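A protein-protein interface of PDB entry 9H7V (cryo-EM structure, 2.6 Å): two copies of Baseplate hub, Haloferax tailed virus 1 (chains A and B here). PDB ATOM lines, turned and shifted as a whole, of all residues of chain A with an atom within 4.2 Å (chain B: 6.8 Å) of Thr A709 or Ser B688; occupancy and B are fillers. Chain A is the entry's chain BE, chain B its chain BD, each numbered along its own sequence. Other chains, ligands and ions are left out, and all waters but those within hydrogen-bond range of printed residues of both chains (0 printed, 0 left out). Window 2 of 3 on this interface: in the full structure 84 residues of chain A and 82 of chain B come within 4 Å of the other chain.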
ATOM      1  N   VAL A 690      25.944  -2.533  16.595  1.00  0.00           N
ATOM      2  CA  VAL A 690      24.686  -1.801  16.655  1.00  0.00           C
ATOM      3  C   VAL A 690      24.547  -0.964  15.379  1.00  0.00           C
ATOM      4  O   VAL A 690      24.974   0.190  15.351  1.00  0.00           O
ATOM      5  CB  VAL A 690      24.605  -0.941  17.938  1.00  0.00           C
ATOM      6  CG1 VAL A 690      23.269  -0.228  18.074  1.00  0.00           C
ATOM      7  CG2 VAL A 690      24.899  -1.737  19.204  1.00  0.00           C
ATOM      8  N   PRO A 691      23.984  -1.514  14.274  1.00  0.00           N
ATOM      9  CA  PRO A 691      23.913  -0.791  12.999  1.00  0.00           C
ATOM     10  C   PRO A 691      22.819   0.267  12.838  1.00  0.00           C
ATOM     11  O   PRO A 691      22.882   1.075  11.914  1.00  0.00           O
ATOM     12  CB  PRO A 691      23.687  -1.921  11.982  1.00  0.00           C
ATOM     13  CG  PRO A 691      22.904  -2.957  12.754  1.00  0.00           C
ATOM     14  CD  PRO A 691      23.447  -2.882  14.166  1.00  0.00           C
ATOM     15  N   ASN A 708      27.110  -0.972   6.363  1.00  0.00           N
ATOM     16  CA  ASN A 708      26.525   0.358   6.481  1.00  0.00           C
ATOM     17  C   ASN A 708      25.982   0.536   7.896  1.00  0.00           C
ATOM     18  O   ASN A 708      25.764  -0.452   8.596  1.00  0.00           O
ATOM     19  CB  ASN A 708      25.427   0.602   5.440  1.00  0.00           C
ATOM     20  CG  ASN A 708      25.937   0.636   4.014  1.00  0.00           C
ATOM     21  OD1 ASN A 708      26.163   1.708   3.456  1.00  0.00           O
ATOM     22  ND2 ASN A 708      26.115  -0.530   3.414  1.00  0.00           N
ATOM     23  N   THR A 709      25.769   1.795   8.314  1.00  0.00           N
ATOM     24  CA  THR A 709      25.087   2.081   9.571  1.00  0.00           C
ATOM     25  C   THR A 709      24.244   3.350   9.464  1.00  0.00           C
ATOM     26  O   THR A 709      24.546   4.252   8.682  1.00  0.00           O
ATOM     27  CB  THR A 709      26.030   2.046  10.783  1.00  0.00           C
ATOM     28  OG1 THR A 709      25.248   2.120  11.975  1.00  0.00           O
ATOM     29  CG2 THR A 709      27.026   3.184  10.797  1.00  0.00           C
ATOM     30  N   PHE A 710      23.192   3.386  10.291  1.00  0.00           N
ATOM     31  CA  PHE A 710      22.144   4.391  10.260  1.00  0.00           C
ATOM     32  C   PHE A 710      21.911   4.872  11.689  1.00  0.00           C
ATOM     33  O   PHE A 710      21.112   4.289  12.420  1.00  0.00           O
ATOM     34  CB  PHE A 710      20.879   3.797   9.627  1.00  0.00           C
ATOM     35  CG  PHE A 710      21.108   3.008   8.360  1.00  0.00           C
ATOM     36  CD1 PHE A 710      21.141   3.646   7.127  1.00  0.00           C
ATOM     37  CD2 PHE A 710      21.304   1.632   8.397  1.00  0.00           C
ATOM     38  CE1 PHE A 710      21.362   2.927   5.961  1.00  0.00           C
ATOM     39  CE2 PHE A 710      21.527   0.913   7.229  1.00  0.00           C
ATOM     40  CZ  PHE A 710      21.554   1.562   6.013  1.00  0.00           C
ATOM     41  N   GLY A 711      22.670   5.897  12.097  1.00  0.00           N
ATOM     42  CA  GLY A 711      22.599   6.456  13.440  1.00  0.00           C
ATOM     43  C   GLY A 711      23.077   5.490  14.525  1.00  0.00           C
ATOM     44  O   GLY A 711      22.889   5.754  15.712  1.00  0.00           O
ATOM     45  N   GLY A 712      23.708   4.383  14.106  1.00  0.00           N
ATOM     46  CA  GLY A 712      24.151   3.321  14.998  1.00  0.00           C
ATOM     47  C   GLY A 712      25.428   3.677  15.760  1.00  0.00           C
ATOM     48  O   GLY A 712      25.972   4.769  15.596  1.00  0.00           O
ATOM     49  N   THR A 715      29.813  -0.975  13.920  1.00  0.00           N
ATOM     50  CA  THR A 715      29.592  -1.879  12.793  1.00  0.00           C
ATOM     51  C   THR A 715      30.440  -3.140  12.957  1.00  0.00           C
ATOM     52  O   THR A 715      31.170  -3.265  13.940  1.00  0.00           O
ATOM     53  CB  THR A 715      29.795  -1.190  11.435  1.00  0.00           C
ATOM     54  OG1 THR A 715      31.174  -0.857  11.265  1.00  0.00           O
ATOM     55  CG2 THR A 715      28.932   0.038  11.248  1.00  0.00           C
ATOM     56  N   THR B 677      23.431  16.427   9.826  1.00  0.00           N
ATOM     57  CA  THR B 677      23.748  15.023   9.612  1.00  0.00           C
ATOM     58  C   THR B 677      25.074  14.921   8.863  1.00  0.00           C
ATOM     59  O   THR B 677      25.308  15.661   7.907  1.00  0.00           O
ATOM     60  CB  THR B 677      22.632  14.318   8.826  1.00  0.00           C
ATOM     61  OG1 THR B 677      21.440  14.401   9.605  1.00  0.00           O
ATOM     62  CG2 THR B 677      22.919  12.863   8.518  1.00  0.00           C
ATOM     63  N   VAL B 678      25.926  13.989   9.308  1.00  0.00           N
ATOM     64  CA  VAL B 678      27.198  13.721   8.657  1.00  0.00           C
ATOM     65  C   VAL B 678      27.159  12.308   8.076  1.00  0.00           C
ATOM     66  O   VAL B 678      26.876  11.347   8.791  1.00  0.00           O
ATOM     67  CB  VAL B 678      28.392  13.923   9.614  1.00  0.00           C
ATOM     68  CG1 VAL B 678      29.720  13.742   8.897  1.00  0.00           C
ATOM     69  CG2 VAL B 678      28.359  15.282  10.297  1.00  0.00           C
ATOM     70  N   THR B 679      27.441  12.207   6.770  1.00  0.00           N
ATOM     71  CA  THR B 679      27.545  10.934   6.071  1.00  0.00           C
ATOM     72  C   THR B 679      28.992  10.717   5.639  1.00  0.00           C
ATOM     73  O   THR B 679      29.566  11.550   4.937  1.00  0.00           O
ATOM     74  CB  THR B 679      26.551  10.851   4.903  1.00  0.00           C
ATOM     75  OG1 THR B 679      25.234  10.918   5.451  1.00  0.00           O
ATOM     76  CG2 THR B 679      26.681   9.584   4.084  1.00  0.00           C
ATOM     77  N   LEU B 680      29.564   9.589   6.075  1.00  0.00           N
ATOM     78  CA  LEU B 680      30.907   9.194   5.685  1.00  0.00           C
ATOM     79  C   LEU B 680      30.830   7.939   4.820  1.00  0.00           C
ATOM     80  O   LEU B 680      30.186   6.956   5.188  1.00  0.00           O
ATOM     81  CB  LEU B 680      31.757   8.987   6.943  1.00  0.00           C
ATOM     82  CG  LEU B 680      33.241   8.705   6.711  1.00  0.00           C
ATOM     83  CD1 LEU B 680      34.104   9.579   7.606  1.00  0.00           C
ATOM     84  CD2 LEU B 680      33.551   7.240   6.959  1.00  0.00           C
ATOM     85  N   ASP B 685      30.562   2.116   1.325  1.00  0.00           N
ATOM     86  CA  ASP B 685      30.008   1.854   2.647  1.00  0.00           C
ATOM     87  C   ASP B 685      29.668   3.184   3.316  1.00  0.00           C
ATOM     88  O   ASP B 685      30.559   3.998   3.552  1.00  0.00           O
ATOM     89  CB  ASP B 685      30.978   1.054   3.526  1.00  0.00           C
ATOM     90  CG  ASP B 685      31.259  -0.368   3.066  1.00  0.00           C
ATOM     91  OD1 ASP B 685      30.507  -0.881   2.211  1.00  0.00           O
ATOM     92  OD2 ASP B 685      32.233  -0.960   3.578  1.00  0.00           O
ATOM     93  N   THR B 686      28.379   3.386   3.632  1.00  0.00           N
ATOM     94  CA  THR B 686      27.914   4.645   4.202  1.00  0.00           C
ATOM     95  C   THR B 686      27.641   4.507   5.698  1.00  0.00           C
ATOM     96  O   THR B 686      26.962   3.581   6.138  1.00  0.00           O
ATOM     97  CB  THR B 686      26.718   5.239   3.443  1.00  0.00           C
ATOM     98  OG1 THR B 686      25.615   4.337   3.542  1.00  0.00           O
ATOM     99  CG2 THR B 686      27.015   5.542   1.990  1.00  0.00           C
ATOM    100  N   TYR B 687      28.181   5.474   6.451  1.00  0.00           N
ATOM    101  CA  TYR B 687      28.013   5.636   7.886  1.00  0.00           C
ATOM    102  C   TYR B 687      27.401   7.015   8.120  1.00  0.00           C
ATOM    103  O   TYR B 687      27.995   8.021   7.734  1.00  0.00           O
ATOM    104  CB  TYR B 687      29.370   5.487   8.586  1.00  0.00           C
ATOM    105  CG  TYR B 687      30.117   4.234   8.204  1.00  0.00           C
ATOM    106  CD1 TYR B 687      30.867   4.168   7.037  1.00  0.00           C
ATOM    107  CD2 TYR B 687      30.042   3.095   8.992  1.00  0.00           C
ATOM    108  CE1 TYR B 687      31.526   3.006   6.668  1.00  0.00           C
ATOM    109  CE2 TYR B 687      30.698   1.925   8.641  1.00  0.00           C
ATOM    110  CZ  TYR B 687      31.443   1.882   7.475  1.00  0.00           C
ATOM    111  OH  TYR B 687      32.096   0.737   7.126  1.00  0.00           O
ATOM    112  N   SER B 688      26.205   7.056   8.723  1.00  0.00           N
ATOM    113  CA  SER B 688      25.503   8.315   8.934  1.00  0.00           C
ATOM    114  C   SER B 688      25.227   8.541  10.418  1.00  0.00           C
ATOM    115  O   SER B 688      24.814   7.618  11.119  1.00  0.00           O
ATOM    116  CB  SER B 688      24.240   8.392   8.113  1.00  0.00           C
ATOM    117  OG  SER B 688      24.541   8.414   6.725  1.00  0.00           O
ATOM    118  N   TRP B 689      25.463   9.779  10.878  1.00  0.00           N
ATOM    119  CA  TRP B 689      25.220  10.160  12.263  1.00  0.00           C
ATOM    120  C   TRP B 689      24.779  11.620  12.375  1.00  0.00           C
ATOM    121  O   TRP B 689      24.993  12.406  11.454  1.00  0.00           O
ATOM    122  CB  TRP B 689      26.420   9.804  13.157  1.00  0.00           C
ATOM    123  CG  TRP B 689      27.655  10.647  13.031  1.00  0.00           C
ATOM    124  CD1 TRP B 689      28.031  11.656  13.868  1.00  0.00           C
ATOM    125  CD2 TRP B 689      28.717  10.518  12.063  1.00  0.00           C
ATOM    126  NE1 TRP B 689      29.233  12.181  13.478  1.00  0.00           N
ATOM    127  CE2 TRP B 689      29.679  11.506  12.375  1.00  0.00           C
ATOM    128  CE3 TRP B 689      28.947   9.686  10.957  1.00  0.00           C
ATOM    129  CZ2 TRP B 689      30.846  11.679  11.626  1.00  0.00           C
ATOM    130  CZ3 TRP B 689      30.100   9.858  10.217  1.00  0.00           C
ATOM    131  CH2 TRP B 689      31.036  10.842  10.549  1.00  0.00           C
ATOM    132  N   VAL B 690      24.143  11.957  13.510  1.00  0.00           N
ATOM    133  CA  VAL B 690      23.556  13.270  13.749  1.00  0.00           C
ATOM    134  C   VAL B 690      24.253  13.906  14.955  1.00  0.00           C
ATOM    135  O   VAL B 690      23.814  13.723  16.091  1.00  0.00           O
ATOM    136  CB  VAL B 690      22.022  13.194  13.929  1.00  0.00           C
ATOM    137  CG1 VAL B 690      21.381  14.574  14.009  1.00  0.00           C
ATOM    138  CG2 VAL B 690      21.345  12.368  12.843  1.00  0.00           C
ATOM    139  N   SER B 714      23.569  10.862  17.889  1.00  0.00           N
ATOM    140  CA  SER B 714      24.529   9.791  17.631  1.00  0.00           C
ATOM    141  C   SER B 714      25.886  10.332  17.170  1.00  0.00           C
ATOM    142  O   SER B 714      25.960  11.391  16.548  1.00  0.00           O
ATOM    143  CB  SER B 714      23.976   8.795  16.640  1.00  0.00           C
ATOM    144  OG  SER B 714      24.768   7.616  16.613  1.00  0.00           O
ATOM    145  N   THR B 715      26.946   9.563  17.469  1.00  0.00           N
ATOM    146  CA  THR B 715      28.337   9.884  17.163  1.00  0.00           C
ATOM    147  C   THR B 715      28.817   9.063  15.964  1.00  0.00           C
ATOM    148  O   THR B 715      28.057   8.261  15.424  1.00  0.00           O
ATOM    149  CB  THR B 715      29.245   9.568  18.363  1.00  0.00           C
ATOM    150  OG1 THR B 715      29.019   8.222  18.786  1.00  0.00           O
ATOM    151  CG2 THR B 715      29.067  10.516  19.529  1.00  0.00           C
ATOM    152  N   PRO B 717      30.472   5.968  14.278  1.00  0.00           N
ATOM    153  CA  PRO B 717      30.425   4.567  14.715  1.00  0.00           C
ATOM    154  C   PRO B 717      31.746   3.803  14.867  1.00  0.00           C
ATOM    155  O   PRO B 717      31.740   2.572  14.882  1.00  0.00           O
ATOM    156  CB  PRO B 717      29.549   3.919  13.631  1.00  0.00           C
ATOM    157  CG  PRO B 717      29.875   4.709  12.385  1.00  0.00           C
ATOM    158  CD  PRO B 717      30.043   6.129  12.877  1.00  0.00           C
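Of the printed residues of chain B, Asn A708 touches Asp B685 and Thr B686.
Of chain B, only Thr B686, Tyr B687, Ser B688 and Pro B717 come within 4 Å of Thr A709.
Of the printed residues of chain B, Thr A715 touches Tyr B687.
Val B678 touches none of the printed residues of chain A.
Of the printed residues of chain A, Ser B688 touches Thr A709 and Gly A711.
Val B690 touches none of the printed residues of chain A.
The nearest residue of chain B that does not touch Thr A709 is Trp B689 (6.0 Å).
The nearest residue of chain A that does not touch Ser B688 is Phe A710 (4.04 Å).
The nearest printed residue of chain B that does not touch Gly A712 is Thr B715 (4.1 Å).
The side-chain amide oxygen of Asn A708 is in hydrogen-bond range of the side-chain hydroxyl of Thr B686 (2.7 Å).
O of Thr B686 lies within hydrogen-bond range of N of Thr A709 (3.1 Å).
N of Ser B688 is in hydrogen-bond range of O of Thr A709, at 3.3 Å.
The backbone carbonyl oxygen (O) of Ser B688 sits at hydrogen-bond distance from the backbone NH (N) of Gly A711, 2.9 Å away.
O of Gly A711 is in hydrogen-bond range of OG of Ser B714.
OG of Ser B714 lies within hydrogen-bond range of O of Gly A712, at 3.3 Å.
The side-chain hydroxyl (OG1) of Thr B679 is in hydrogen-bond range of the side-chain hydroxyl (OG) of Ser B688 (2.9 Å).
The backbone carbonyl oxygen of Tyr B687 sits at hydrogen-bond distance from the backbone NH of Leu B680 (2.8 Å).
O of Val B690 lies within hydrogen-bond range of N of Ser B714 (3.4 Å).
The backbone carbonyl oxygen (O) of Pro A691 lies within hydrogen-bond range of the side-chain hydroxyl (OG1) of Thr A709 (2.6 Å).
OG1 of Thr A709 sits close to N of Gly A712 (3.5 Å).
Positions printed for both chains: 690 and 715.
Among the printed residues, pairs that only touch across the chains: Asn A708 with Asp B685 (3.8 Å), Thr A709 with Tyr B687 (3.5 Å), Thr A709 with Pro B717 (3.6 Å) and Thr A715 with Tyr B687 (3.7 Å).
Of the 13 printed residues of chain B, 6 touch a printed residue of chain A.
Printed residues of chain B that touch a printed residue of chain A: Asp B685, Thr B686, Tyr B687, Ser B688, Ser B714 and Pro B717.
Among the printed residues, 10 pairs touch across the chains.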
